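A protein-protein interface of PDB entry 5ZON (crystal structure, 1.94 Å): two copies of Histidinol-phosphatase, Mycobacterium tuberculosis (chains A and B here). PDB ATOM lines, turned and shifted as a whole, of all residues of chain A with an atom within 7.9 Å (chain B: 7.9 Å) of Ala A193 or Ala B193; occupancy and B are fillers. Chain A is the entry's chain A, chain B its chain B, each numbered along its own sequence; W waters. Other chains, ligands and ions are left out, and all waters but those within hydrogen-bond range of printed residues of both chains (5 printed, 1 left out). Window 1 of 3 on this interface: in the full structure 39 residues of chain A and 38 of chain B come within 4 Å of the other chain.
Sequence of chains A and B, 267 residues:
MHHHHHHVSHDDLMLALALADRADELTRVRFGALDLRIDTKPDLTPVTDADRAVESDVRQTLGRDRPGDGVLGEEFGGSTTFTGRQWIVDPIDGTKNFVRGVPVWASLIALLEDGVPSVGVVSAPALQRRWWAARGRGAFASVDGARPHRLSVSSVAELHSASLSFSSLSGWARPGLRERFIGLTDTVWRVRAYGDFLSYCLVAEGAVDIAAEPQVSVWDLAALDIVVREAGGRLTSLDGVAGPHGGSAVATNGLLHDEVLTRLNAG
OD2 of Asp A196 is in salt-bridge range of NH2 of Arg B192 (3.1 Å).
O of Ser B167 lies close to O of Val A191 (3.5 Å).
O of Ser B167 lies within hydrogen-bond range of NH1 of Arg A192.
NH2 of Arg A190 is in salt-bridge range of OD1 of Asp B196, 3.6 Å away.
NH2 of Arg A190 lies within hydrogen-bond range of OD1 of Asn B97.
OD1 of Asp B196 is in salt-bridge range of NH2 of Arg A192 (3.0 Å).
The backbone carbonyl oxygen (O) of Ser A167 sits at hydrogen-bond distance from the guanidinium group (NH1) of Arg B192, 3.4 Å away.
The side-chain amide oxygen (OD1) of Asn B97 lies within hydrogen-bond range of the side-chain hydroxyl (OH) of Tyr A194 (3.3 Å).
O of Ala A193 is in hydrogen-bond range of N of Ala B193, 3.0 Å away.
OG of Ser B167 lies within hydrogen-bond range of N of Asp B196 (3.0 Å).
The backbone NH (N) of Phe B166 is in hydrogen-bond range of the backbone carbonyl oxygen (O) of Arg B192 (3.1 Å).
The backbone NH (N) of Gly A195 is in hydrogen-bond range of the side-chain hydroxyl (OG) of Ser A199, 3.4 Å away.
The side-chain hydroxyl (OG) of Ser B165 sits at hydrogen-bond distance from the backbone NH (N) of Tyr B194 (3.1 Å).
The backbone carbonyl oxygen (O) of Leu B164 sits at hydrogen-bond distance from the backbone NH (N) of Arg B192, at 3.0 Å.
The backbone carbonyl oxygen (O) of Leu A164 sits at hydrogen-bond distance from the backbone NH (N) of Arg A192 (3.0 Å).
Ser A167 touches Val B191.
Ser A168 touches Val B191 (CB to O, 3.7 Å).
Ser A168 touches Arg B192 (CB to NH1, 3.996 Å).
Val A191 touches Ser B168.
CB of Ser B168 touches NH1 of Arg A192, at 3.9 Å.
Arg A192 touches Ala B193.
NE of Arg A192 touches CA of Gly B195, at 3.5 Å.
Ala A193 touches Arg B192.
Tyr A194 touches Tyr B194 (O to CE1, 3.7 Å).
Gly A195 touches Arg B192 (CA to NE, 3.6 Å).
Of chain B, only Arg B192 and Ala B193 come within 4 Å of Ala A193.
Of the printed residues of chain A, Ala B193 touches Arg A192 (3.5 Å) and Ala A193 (3.0 Å).
Of the printed residues of chain A, Ser B167 touches Val A191 (3.5 Å) and Arg A192 (3.4 Å).
Of the printed residues of chain B, Val A191 touches Ser B167 (3.5 Å) and Ser B168 (3.6 Å).
Leu A169 touches none of the printed residues of chain B.
Leu B169 touches none of the printed residues of chain A.
The nearest residue of chain B that does not touch Ala A193 is Tyr B194 (4.1 Å).
The nearest printed residue of chain A that does not touch Ser B168 is Arg A190 (6.2 Å).
Of the 18 printed residues of chain A, 9 touch a printed residue of chain B.
Printed residues of chain A that touch a printed residue of chain B: Ser A167, Ser A168, Arg A190, Val A191, Arg A192, Ala A193, Tyr A194, Gly A195 and Asp A196.
Hydrophobic or aromatic side chains of chain A within 4 Å of the printed part of chain B: Ala A193 and Tyr A194.
Along chain A the printed residues that touch a printed residue of chain B span positions 167 to 196.
Hydrophobic or aromatic side chains of chain B that line the printed part of chain A: Ala B193 and Tyr B194.
Among the printed residues, 19 pairs touch across the chains.
Ser A167 touches Val B191, and with the chains exchanged Val A191 touches Ser B167.
Arg A192 touches Gly B195, and with the chains exchanged Gly A195 touches Arg B192.
Arg A192 touches Asp B196, and with the chains exchanged Asp A196 touches Arg B192.
Ala A193 touches its own counterpart, Ala B193.
17 positions are printed for both chains.
Water W3 lies within hydrogen-bond range of OD1 of Asp A196 (2.6 Å) and NH2 of Arg B192 (3.4 Å).
Water W5 lies within hydrogen-bond range of O of Tyr B194 (2.6 Å), ND2 of Asn B97 (2.9 Å), NE of Arg A192 (3.0 Å), OD1 of Asp B196 (3.1 Å) and OH of Tyr A194 (3.4 Å).
Water W2 lies within hydrogen-bond range of O of Tyr A194 (2.7 Å), NE of Arg B192 (3.0 Å), OH of Tyr B194 (3.0 Å) and OD2 of Asp A196 (3.3 Å).
Water W1 lies within hydrogen-bond range of OH of Tyr A194 (2.8 Å), NE of Arg A190 (3.1 Å) and OD1 of Asn B97 (3.2 Å).
Water W4 lies within hydrogen-bond range of the side-chain amide oxygen (OD1) of Asn B97 (3.1 Å) and the guanidinium group (NE) of Arg A190 (3.3 Å).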
ATOM      1  N   VAL A 104      -4.016 -29.294  14.897  1.00  0.00           N
ATOM      2  CA  VAL A 104      -3.853 -27.806  14.867  1.00  0.00           C
ATOM      3  C   VAL A 104      -5.167 -27.134  15.279  1.00  0.00           C
ATOM      4  O   VAL A 104      -5.958 -26.720  14.441  1.00  0.00           O
ATOM      5  CB  VAL A 104      -3.341 -27.274  13.518  1.00  0.00           C
ATOM      6  CG1 VAL A 104      -3.111 -25.750  13.539  1.00  0.00           C
ATOM      7  CG2 VAL A 104      -2.063 -28.004  13.095  1.00  0.00           C
ATOM      8  N   LEU A 164       6.903 -16.916   5.383  1.00  0.00           N
ATOM      9  CA  LEU A 164       5.502 -16.535   5.504  1.00  0.00           C
ATOM     10  C   LEU A 164       4.629 -17.778   5.778  1.00  0.00           C
ATOM     11  O   LEU A 164       4.833 -18.837   5.197  1.00  0.00           O
ATOM     12  CB  LEU A 164       5.115 -15.859   4.182  1.00  0.00           C
ATOM     13  CG  LEU A 164       3.634 -15.813   3.808  1.00  0.00           C
ATOM     14  CD1 LEU A 164       2.895 -14.714   4.566  1.00  0.00           C
ATOM     15  CD2 LEU A 164       3.496 -15.618   2.293  1.00  0.00           C
ATOM     16  N   SER A 165       3.627 -17.639   6.642  1.00  0.00           N
ATOM     17  CA  SER A 165       2.606 -18.692   6.834  1.00  0.00           C
ATOM     18  C   SER A 165       1.226 -18.046   6.736  1.00  0.00           C
ATOM     19  O   SER A 165       1.010 -16.977   7.295  1.00  0.00           O
ATOM     20  CB  SER A 165       2.756 -19.446   8.137  1.00  0.00           C
ATOM     21  OG  SER A 165       1.726 -20.419   8.305  1.00  0.00           O
ATOM     22  N   PHE A 166       0.324 -18.683   5.987  1.00  0.00           N
ATOM     23  CA  PHE A 166      -1.047 -18.178   5.826  1.00  0.00           C
ATOM     24  C   PHE A 166      -2.021 -19.323   6.136  1.00  0.00           C
ATOM     25  O   PHE A 166      -1.613 -20.336   6.744  1.00  0.00           O
ATOM     26  CB  PHE A 166      -1.207 -17.534   4.441  1.00  0.00           C
ATOM     27  CG  PHE A 166      -1.149 -18.437   3.226  1.00  0.00           C
ATOM     28  CD1 PHE A 166       0.056 -18.926   2.750  1.00  0.00           C
ATOM     29  CD2 PHE A 166      -2.304 -18.740   2.499  1.00  0.00           C
ATOM     30  CE1 PHE A 166       0.110 -19.722   1.606  1.00  0.00           C
ATOM     31  CE2 PHE A 166      -2.255 -19.526   1.347  1.00  0.00           C
ATOM     32  CZ  PHE A 166      -1.041 -20.010   0.901  1.00  0.00           C
ATOM     33  N   SER A 167      -3.291 -19.155   5.733  1.00  0.00           N
ATOM     34  CA  SER A 167      -4.267 -20.227   5.879  1.00  0.00           C
ATOM     35  C   SER A 167      -4.603 -20.812   4.490  1.00  0.00           C
ATOM     36  O   SER A 167      -4.169 -21.898   4.151  1.00  0.00           O
ATOM     37  CB  SER A 167      -5.484 -19.743   6.631  1.00  0.00           C
ATOM     38  OG  SER A 167      -5.183 -19.610   8.022  1.00  0.00           O
ATOM     39  N   SER A 168      -5.382 -20.116   3.675  1.00  0.00           N
ATOM     40  CA  SER A 168      -5.618 -20.578   2.325  1.00  0.00           C
ATOM     41  C   SER A 168      -5.763 -19.377   1.387  1.00  0.00           C
ATOM     42  O   SER A 168      -5.810 -18.224   1.830  1.00  0.00           O
ATOM     43  CB  SER A 168      -6.847 -21.469   2.246  1.00  0.00           C
ATOM     44  OG  SER A 168      -8.007 -20.763   2.681  1.00  0.00           O
ATOM     45  N   LEU A 169      -5.870 -19.687   0.099  1.00  0.00           N
ATOM     46  CA  LEU A 169      -5.911 -18.665  -0.942  1.00  0.00           C
ATOM     47  C   LEU A 169      -7.325 -18.116  -1.070  1.00  0.00           C
ATOM     48  O   LEU A 169      -7.501 -16.955  -1.356  1.00  0.00           O
ATOM     49  CB  LEU A 169      -5.447 -19.280  -2.268  1.00  0.00           C
ATOM     50  CG  LEU A 169      -3.928 -19.409  -2.445  1.00  0.00           C
ATOM     51  CD1 LEU A 169      -3.164 -18.314  -1.719  1.00  0.00           C
ATOM     52  CD2 LEU A 169      -3.409 -20.781  -2.036  1.00  0.00           C
ATOM     53  N   PHE A 181      -1.630 -11.051  -3.053  1.00  0.00           N
ATOM     54  CA  PHE A 181      -1.159 -12.015  -2.054  1.00  0.00           C
ATOM     55  C   PHE A 181      -0.228 -13.039  -2.711  1.00  0.00           C
ATOM     56  O   PHE A 181       0.843 -13.359  -2.172  1.00  0.00           O
ATOM     57  CB  PHE A 181      -2.320 -12.717  -1.342  1.00  0.00           C
ATOM     58  CG  PHE A 181      -1.818 -13.646  -0.264  1.00  0.00           C
ATOM     59  CD1 PHE A 181      -1.191 -13.145   0.878  1.00  0.00           C
ATOM     60  CD2 PHE A 181      -1.875 -15.014  -0.438  1.00  0.00           C
ATOM     61  CE1 PHE A 181      -0.670 -13.992   1.843  1.00  0.00           C
ATOM     62  CE2 PHE A 181      -1.336 -15.854   0.517  1.00  0.00           C
ATOM     63  CZ  PHE A 181      -0.746 -15.347   1.664  1.00  0.00           C
ATOM     64  N   ARG A 190      10.343 -18.293   1.900  1.00  0.00           N
ATOM     65  CA  ARG A 190       9.691 -19.575   2.202  1.00  0.00           C
ATOM     66  C   ARG A 190       8.198 -19.319   2.464  1.00  0.00           C
ATOM     67  O   ARG A 190       7.854 -18.354   3.160  1.00  0.00           O
ATOM     68  CB  ARG A 190      10.332 -20.193   3.453  1.00  0.00           C
ATOM     69  CG  ARG A 190       9.718 -21.541   3.806  1.00  0.00           C
ATOM     70  CD  ARG A 190      10.514 -22.321   4.815  1.00  0.00           C
ATOM     71  NE  ARG A 190       9.878 -23.592   5.161  1.00  0.00           N
ATOM     72  CZ  ARG A 190      10.133 -24.747   4.560  1.00  0.00           C
ATOM     73  NH1 ARG A 190      10.751 -24.767   3.387  1.00  0.00           N
ATOM     74  NH2 ARG A 190       9.742 -25.872   5.121  1.00  0.00           N
ATOM     75  N   VAL A 191       7.348 -20.195   1.916  1.00  0.00           N
ATOM     76  CA  VAL A 191       5.888 -20.119   2.111  1.00  0.00           C
ATOM     77  C   VAL A 191       5.387 -21.467   2.653  1.00  0.00           C
ATOM     78  O   VAL A 191       5.706 -22.530   2.101  1.00  0.00           O
ATOM     79  CB  VAL A 191       5.158 -19.790   0.786  1.00  0.00           C
ATOM     80  CG1 VAL A 191       3.683 -19.517   1.051  1.00  0.00           C
ATOM     81  CG2 VAL A 191       5.773 -18.592   0.063  1.00  0.00           C
ATOM     82  N   ARG A 192       4.545 -21.399   3.673  1.00  0.00           N
ATOM     83  CA  ARG A 192       3.778 -22.544   4.187  1.00  0.00           C
ATOM     84  C   ARG A 192       2.387 -22.018   4.565  1.00  0.00           C
ATOM     85  O   ARG A 192       2.172 -20.786   4.557  1.00  0.00           O
ATOM     86  CB  ARG A 192       4.480 -23.147   5.419  1.00  0.00           C
ATOM     87  CG  ARG A 192       5.686 -24.028   5.093  1.00  0.00           C
ATOM     88  CD  ARG A 192       5.298 -25.206   4.194  1.00  0.00           C
ATOM     89  NE  ARG A 192       6.400 -26.118   3.889  1.00  0.00           N
ATOM     90  CZ  ARG A 192       7.162 -26.048   2.794  1.00  0.00           C
ATOM     91  NH1 ARG A 192       6.982 -25.075   1.912  1.00  0.00           N
ATOM     92  NH2 ARG A 192       8.091 -26.970   2.592  1.00  0.00           N
ATOM     93  N   ALA A 193       1.450 -22.921   4.885  1.00  0.00           N
ATOM     94  CA  ALA A 193       0.150 -22.504   5.413  1.00  0.00           C
ATOM     95  C   ALA A 193      -0.221 -23.424   6.589  1.00  0.00           C
ATOM     96  O   ALA A 193      -0.934 -24.415   6.429  1.00  0.00           O
ATOM     97  CB  ALA A 193      -0.862 -22.477   4.272  1.00  0.00           C
ATOM     98  N   TYR A 194       0.319 -23.119   7.773  1.00  0.00           N
ATOM     99  CA  TYR A 194       0.068 -23.876   9.000  1.00  0.00           C
ATOM    100  C   TYR A 194      -1.356 -23.577   9.486  1.00  0.00           C
ATOM    101  O   TYR A 194      -1.957 -24.383  10.221  1.00  0.00           O
ATOM    102  CB  TYR A 194       1.147 -23.585  10.058  1.00  0.00           C
ATOM    103  CG  TYR A 194       2.549 -23.923   9.593  1.00  0.00           C
ATOM    104  CD1 TYR A 194       2.910 -25.224   9.263  1.00  0.00           C
ATOM    105  CD2 TYR A 194       3.514 -22.925   9.452  1.00  0.00           C
ATOM    106  CE1 TYR A 194       4.188 -25.527   8.803  1.00  0.00           C
ATOM    107  CE2 TYR A 194       4.806 -23.215   9.024  1.00  0.00           C
ATOM    108  CZ  TYR A 194       5.135 -24.522   8.691  1.00  0.00           C
ATOM    109  OH  TYR A 194       6.389 -24.815   8.249  1.00  0.00           O
ATOM    110  N   GLY A 195      -1.867 -22.409   9.093  1.00  0.00           N
ATOM    111  CA  GLY A 195      -3.267 -22.067   9.261  1.00  0.00           C
ATOM    112  C   GLY A 195      -3.603 -21.562  10.658  1.00  0.00           C
ATOM    113  O   GLY A 195      -2.919 -21.888  11.677  1.00  0.00           O
ATOM    114  N   ASP A 196      -4.667 -20.758  10.714  1.00  0.00           N
ATOM    115  CA  ASP A 196      -5.323 -20.353  11.989  1.00  0.00           C
ATOM    116  C   ASP A 196      -4.306 -19.676  12.924  1.00  0.00           C
ATOM    117  O   ASP A 196      -3.421 -18.941  12.451  1.00  0.00           O
ATOM    118  CB  ASP A 196      -6.085 -21.531  12.605  1.00  0.00           C
ATOM    119  CG  ASP A 196      -7.079 -22.188  11.642  1.00  0.00           C
ATOM    120  OD1 ASP A 196      -8.239 -21.675  11.535  1.00  0.00           O
ATOM    121  OD2 ASP A 196      -6.692 -23.205  11.001  1.00  0.00           O
ATOM    122  N   LEU A 198      -1.847 -20.837  14.481  1.00  0.00           N
ATOM    123  CA  LEU A 198      -0.494 -21.382  14.549  1.00  0.00           C
ATOM    124  C   LEU A 198       0.486 -20.488  13.768  1.00  0.00           C
ATOM    125  O   LEU A 198       1.616 -20.281  14.228  1.00  0.00           O
ATOM    126  CB  LEU A 198      -0.475 -22.835  14.042  1.00  0.00           C
ATOM    127  CG  LEU A 198       0.872 -23.560  14.150  1.00  0.00           C
ATOM    128  CD1 LEU A 198       1.435 -23.491  15.581  1.00  0.00           C
ATOM    129  CD2 LEU A 198       0.708 -25.020  13.677  1.00  0.00           C
ATOM    130  N   SER A 199       0.070 -19.945  12.620  1.00  0.00           N
ATOM    131  CA  SER A 199       0.893 -18.993  11.841  1.00  0.00           C
ATOM    132  C   SER A 199       1.400 -17.850  12.750  1.00  0.00           C
ATOM    133  O   SER A 199       2.586 -17.485  12.714  1.00  0.00           O
ATOM    134  CB  SER A 199       0.100 -18.452  10.670  1.00  0.00           C
ATOM    135  OG  SER A 199      -0.211 -19.489   9.721  1.00  0.00           O
ATOM    136  N   LEU A 202       3.895 -18.860  15.588  1.00  0.00           N
ATOM    137  CA  LEU A 202       5.227 -19.062  15.012  1.00  0.00           C
ATOM    138  C   LEU A 202       5.900 -17.711  14.704  1.00  0.00           C
ATOM    139  O   LEU A 202       7.138 -17.604  14.820  1.00  0.00           O
ATOM    140  CB  LEU A 202       5.067 -19.919  13.753  1.00  0.00           C
ATOM    141  CG  LEU A 202       4.770 -21.403  14.011  1.00  0.00           C
ATOM    142  CD1 LEU A 202       4.583 -22.124  12.675  1.00  0.00           C
ATOM    143  CD2 LEU A 202       5.901 -22.079  14.789  1.00  0.00           C
ATOM    144  N   ASN B  97      12.871 -25.924   8.053  1.00  0.00           N
ATOM    145  CA  ASN B  97      12.064 -25.717   9.266  1.00  0.00           C
ATOM    146  C   ASN B  97      12.962 -25.885  10.504  1.00  0.00           C
ATOM    147  O   ASN B  97      12.944 -25.088  11.426  1.00  0.00           O
ATOM    148  CB  ASN B  97      10.915 -26.736   9.358  1.00  0.00           C
ATOM    149  CG  ASN B  97       9.789 -26.466   8.375  1.00  0.00           C
ATOM    150  OD1 ASN B  97       9.613 -25.343   7.903  1.00  0.00           O
ATOM    151  ND2 ASN B  97       9.029 -27.496   8.050  1.00  0.00           N
ATOM    152  N   VAL B 104       8.274 -28.919  12.404  1.00  0.00           N
ATOM    153  CA  VAL B 104       7.881 -29.847  11.299  1.00  0.00           C
ATOM    154  C   VAL B 104       9.156 -30.313  10.589  1.00  0.00           C
ATOM    155  O   VAL B 104       9.540 -29.788   9.560  1.00  0.00           O
ATOM    156  CB  VAL B 104       6.870 -29.206  10.316  1.00  0.00           C
ATOM    157  CG1 VAL B 104       6.423 -30.172   9.227  1.00  0.00           C
ATOM    158  CG2 VAL B 104       5.654 -28.637  11.029  1.00  0.00           C
ATOM    159  N   LEU B 164      -6.886 -31.061   1.340  1.00  0.00           N
ATOM    160  CA  LEU B 164      -5.598 -31.132   0.662  1.00  0.00           C
ATOM    161  C   LEU B 164      -4.500 -30.445   1.506  1.00  0.00           C
ATOM    162  O   LEU B 164      -4.730 -29.375   2.085  1.00  0.00           O
ATOM    163  CB  LEU B 164      -5.759 -30.433  -0.690  1.00  0.00           C
ATOM    164  CG  LEU B 164      -4.475 -30.436  -1.513  1.00  0.00           C
ATOM    165  CD1 LEU B 164      -4.780 -30.755  -2.952  1.00  0.00           C
ATOM    166  CD2 LEU B 164      -3.671 -29.152  -1.377  1.00  0.00           C
ATOM    167  N   SER B 165      -3.315 -31.038   1.591  1.00  0.00           N
ATOM    168  CA  SER B 165      -2.123 -30.345   2.130  1.00  0.00           C
ATOM    169  C   SER B 165      -0.989 -30.403   1.100  1.00  0.00           C
ATOM    170  O   SER B 165      -0.757 -31.448   0.484  1.00  0.00           O
ATOM    171  CB  SER B 165      -1.694 -30.917   3.457  1.00  0.00           C
ATOM    172  OG  SER B 165      -0.546 -30.247   3.983  1.00  0.00           O
ATOM    173  N   PHE B 166      -0.330 -29.280   0.880  1.00  0.00           N
ATOM    174  CA  PHE B 166       0.822 -29.212  -0.056  1.00  0.00           C
ATOM    175  C   PHE B 166       2.016 -28.586   0.682  1.00  0.00           C
ATOM    176  O   PHE B 166       2.009 -28.527   1.921  1.00  0.00           O
ATOM    177  CB  PHE B 166       0.411 -28.533  -1.367  1.00  0.00           C
ATOM    178  CG  PHE B 166       0.094 -27.049  -1.313  1.00  0.00           C
ATOM    179  CD1 PHE B 166      -1.110 -26.589  -0.794  1.00  0.00           C
ATOM    180  CD2 PHE B 166       0.975 -26.106  -1.854  1.00  0.00           C
ATOM    181  CE1 PHE B 166      -1.416 -25.232  -0.779  1.00  0.00           C
ATOM    182  CE2 PHE B 166       0.674 -24.748  -1.821  1.00  0.00           C
ATOM    183  CZ  PHE B 166      -0.534 -24.311  -1.321  1.00  0.00           C
ATOM    184  N   SER B 167       3.024 -28.149  -0.060  1.00  0.00           N
ATOM    185  CA  SER B 167       4.159 -27.434   0.501  1.00  0.00           C
ATOM    186  C   SER B 167       4.106 -25.957   0.079  1.00  0.00           C
ATOM    187  O   SER B 167       3.739 -25.097   0.871  1.00  0.00           O
ATOM    188  CB  SER B 167       5.463 -28.108   0.131  1.00  0.00           C
ATOM    189  OG  SER B 167       5.605 -29.328   0.878  1.00  0.00           O
ATOM    190  N   SER B 168       4.462 -25.637  -1.160  1.00  0.00           N
ATOM    191  CA  SER B 168       4.316 -24.266  -1.619  1.00  0.00           C
ATOM    192  C   SER B 168       3.902 -24.233  -3.086  1.00  0.00           C
ATOM    193  O   SER B 168       3.883 -25.265  -3.762  1.00  0.00           O
ATOM    194  CB  SER B 168       5.561 -23.457  -1.384  1.00  0.00           C
ATOM    195  OG  SER B 168       6.650 -23.998  -2.101  1.00  0.00           O
ATOM    196  N   LEU B 169       3.592 -23.030  -3.552  1.00  0.00           N
ATOM    197  CA  LEU B 169       3.083 -22.832  -4.905  1.00  0.00           C
ATOM    198  C   LEU B 169       4.270 -22.772  -5.866  1.00  0.00           C
ATOM    199  O   LEU B 169       4.178 -23.224  -6.996  1.00  0.00           O
ATOM    200  CB  LEU B 169       2.286 -21.525  -4.986  1.00  0.00           C
ATOM    201  CG  LEU B 169       0.962 -21.487  -4.228  1.00  0.00           C
ATOM    202  CD1 LEU B 169       0.319 -20.112  -4.270  1.00  0.00           C
ATOM    203  CD2 LEU B 169       0.021 -22.559  -4.746  1.00  0.00           C
ATOM    204  N   PHE B 181      -2.758 -26.694 -10.633  1.00  0.00           N
ATOM    205  CA  PHE B 181      -2.687 -26.968  -9.180  1.00  0.00           C
ATOM    206  C   PHE B 181      -3.619 -26.009  -8.426  1.00  0.00           C
ATOM    207  O   PHE B 181      -4.372 -26.424  -7.539  1.00  0.00           O
ATOM    208  CB  PHE B 181      -1.254 -26.893  -8.638  1.00  0.00           C
ATOM    209  CG  PHE B 181      -1.198 -27.212  -7.164  1.00  0.00           C
ATOM    210  CD1 PHE B 181      -1.469 -28.497  -6.709  1.00  0.00           C
ATOM    211  CD2 PHE B 181      -1.000 -26.205  -6.221  1.00  0.00           C
ATOM    212  CE1 PHE B 181      -1.493 -28.790  -5.351  1.00  0.00           C
ATOM    213  CE2 PHE B 181      -1.020 -26.496  -4.862  1.00  0.00           C
ATOM    214  CZ  PHE B 181      -1.257 -27.791  -4.434  1.00  0.00           C
ATOM    215  N   VAL B 191      -7.949 -26.457   2.150  1.00  0.00           N
ATOM    216  CA  VAL B 191      -6.551 -26.366   1.689  1.00  0.00           C
ATOM    217  C   VAL B 191      -5.684 -25.858   2.848  1.00  0.00           C
ATOM    218  O   VAL B 191      -6.017 -24.868   3.499  1.00  0.00           O
ATOM    219  CB  VAL B 191      -6.390 -25.426   0.471  1.00  0.00           C
ATOM    220  CG1 VAL B 191      -4.956 -25.495  -0.076  1.00  0.00           C
ATOM    221  CG2 VAL B 191      -7.388 -25.741  -0.635  1.00  0.00           C
ATOM    222  N   ARG B 192      -4.567 -26.531   3.067  1.00  0.00           N
ATOM    223  CA  ARG B 192      -3.518 -26.126   4.006  1.00  0.00           C
ATOM    224  C   ARG B 192      -2.182 -26.497   3.360  1.00  0.00           C
ATOM    225  O   ARG B 192      -2.186 -27.221   2.334  1.00  0.00           O
ATOM    226  CB  ARG B 192      -3.674 -26.855   5.344  1.00  0.00           C
ATOM    227  CG  ARG B 192      -4.763 -26.264   6.244  1.00  0.00           C
ATOM    228  CD  ARG B 192      -4.527 -24.791   6.565  1.00  0.00           C
ATOM    229  NE  ARG B 192      -5.544 -24.253   7.453  1.00  0.00           N
ATOM    230  CZ  ARG B 192      -6.544 -23.475   7.067  1.00  0.00           C
ATOM    231  NH1 ARG B 192      -6.788 -23.329   5.782  1.00  0.00           N
ATOM    232  NH2 ARG B 192      -7.329 -22.887   7.966  1.00  0.00           N
ATOM    233  N   ALA B 193      -1.063 -26.005   3.920  1.00  0.00           N
ATOM    234  CA  ALA B 193       0.251 -26.450   3.436  1.00  0.00           C
ATOM    235  C   ALA B 193       1.169 -26.725   4.649  1.00  0.00           C
ATOM    236  O   ALA B 193       1.964 -25.869   5.054  1.00  0.00           O
ATOM    237  CB  ALA B 193       0.791 -25.411   2.465  1.00  0.00           C
ATOM    238  N   TYR B 194       1.002 -27.895   5.267  1.00  0.00           N
ATOM    239  CA  TYR B 194       1.783 -28.296   6.444  1.00  0.00           C
ATOM    240  C   TYR B 194       3.204 -28.653   5.984  1.00  0.00           C
ATOM    241  O   TYR B 194       4.152 -28.591   6.765  1.00  0.00           O
ATOM    242  CB  TYR B 194       1.108 -29.451   7.203  1.00  0.00           C
ATOM    243  CG  TYR B 194      -0.303 -29.153   7.652  1.00  0.00           C
ATOM    244  CD1 TYR B 194      -0.557 -28.124   8.550  1.00  0.00           C
ATOM    245  CD2 TYR B 194      -1.397 -29.852   7.146  1.00  0.00           C
ATOM    246  CE1 TYR B 194      -1.856 -27.804   8.930  1.00  0.00           C
ATOM    247  CE2 TYR B 194      -2.692 -29.574   7.551  1.00  0.00           C
ATOM    248  CZ  TYR B 194      -2.921 -28.540   8.446  1.00  0.00           C
ATOM    249  OH  TYR B 194      -4.188 -28.212   8.829  1.00  0.00           O
ATOM    250  N   GLY B 195       3.343 -29.019   4.721  1.00  0.00           N
ATOM    251  CA  GLY B 195       4.645 -29.106   4.069  1.00  0.00           C
ATOM    252  C   GLY B 195       5.336 -30.442   4.322  1.00  0.00           C
ATOM    253  O   GLY B 195       5.083 -31.148   5.349  1.00  0.00           O
ATOM    254  N   ASP B 196       6.228 -30.789   3.394  1.00  0.00           N
ATOM    255  CA  ASP B 196       7.191 -31.907   3.581  1.00  0.00           C
ATOM    256  C   ASP B 196       6.454 -33.225   3.875  1.00  0.00           C
ATOM    257  O   ASP B 196       5.373 -33.471   3.343  1.00  0.00           O
ATOM    258  CB  ASP B 196       8.277 -31.529   4.604  1.00  0.00           C
ATOM    259  CG  ASP B 196       9.007 -30.247   4.241  1.00  0.00           C
ATOM    260  OD1 ASP B 196       8.511 -29.164   4.594  1.00  0.00           O
ATOM    261  OD2 ASP B 196      10.067 -30.340   3.603  1.00  0.00           O
ATOM    262  N   LEU B 198       4.858 -34.120   6.412  1.00  0.00           N
ATOM    263  CA  LEU B 198       3.696 -34.100   7.298  1.00  0.00           C
ATOM    264  C   LEU B 198       2.402 -34.229   6.497  1.00  0.00           C
ATOM    265  O   LEU B 198       1.497 -34.929   6.948  1.00  0.00           O
ATOM    266  CB  LEU B 198       3.704 -32.818   8.142  1.00  0.00           C
ATOM    267  CG  LEU B 198       2.623 -32.718   9.223  1.00  0.00           C
ATOM    268  CD1 LEU B 198       2.585 -33.967  10.106  1.00  0.00           C
ATOM    269  CD2 LEU B 198       2.835 -31.455  10.074  1.00  0.00           C
ATOM    270  N   SER B 199       2.307 -33.591   5.331  1.00  0.00           N
ATOM    271  CA  SER B 199       1.154 -33.729   4.426  1.00  0.00           C
ATOM    272  C   SER B 199       0.818 -35.213   4.186  1.00  0.00           C
ATOM    273  O   SER B 199      -0.347 -35.616   4.262  1.00  0.00           O
ATOM    274  CB  SER B 199       1.442 -33.025   3.105  1.00  0.00           C
ATOM    275  OG  SER B 199       1.600 -31.607   3.270  1.00  0.00           O
ATOM    276  N   LEU B 202      -0.394 -37.241   7.282  1.00  0.00           N
ATOM    277  CA  LEU B 202      -1.797 -36.905   7.569  1.00  0.00           C
ATOM    278  C   LEU B 202      -2.732 -37.623   6.573  1.00  0.00           C
ATOM    279  O   LEU B 202      -3.839 -38.019   6.936  1.00  0.00           O
ATOM    280  CB  LEU B 202      -1.945 -35.383   7.502  1.00  0.00           C
ATOM    281  CG  LEU B 202      -1.328 -34.595   8.665  1.00  0.00           C
ATOM    282  CD1 LEU B 202      -1.438 -33.078   8.424  1.00  0.00           C
ATOM    283  CD2 LEU B 202      -2.020 -34.960   9.970  1.00  0.00           C
HETATM  284  O   HOH W   1       7.916 -22.642   7.348  1.00  0.00           O
HETATM  285  O   HOH W   2      -4.475 -25.397   9.960  1.00  0.00           O
HETATM  286  O   HOH W   3      -9.794 -23.378  10.272  1.00  0.00           O
HETATM  287  O   HOH W   4      11.157 -22.677   8.009  1.00  0.00           O
HETATM  288  O   HOH W   5       6.600 -27.656   6.467  1.00  0.00           O
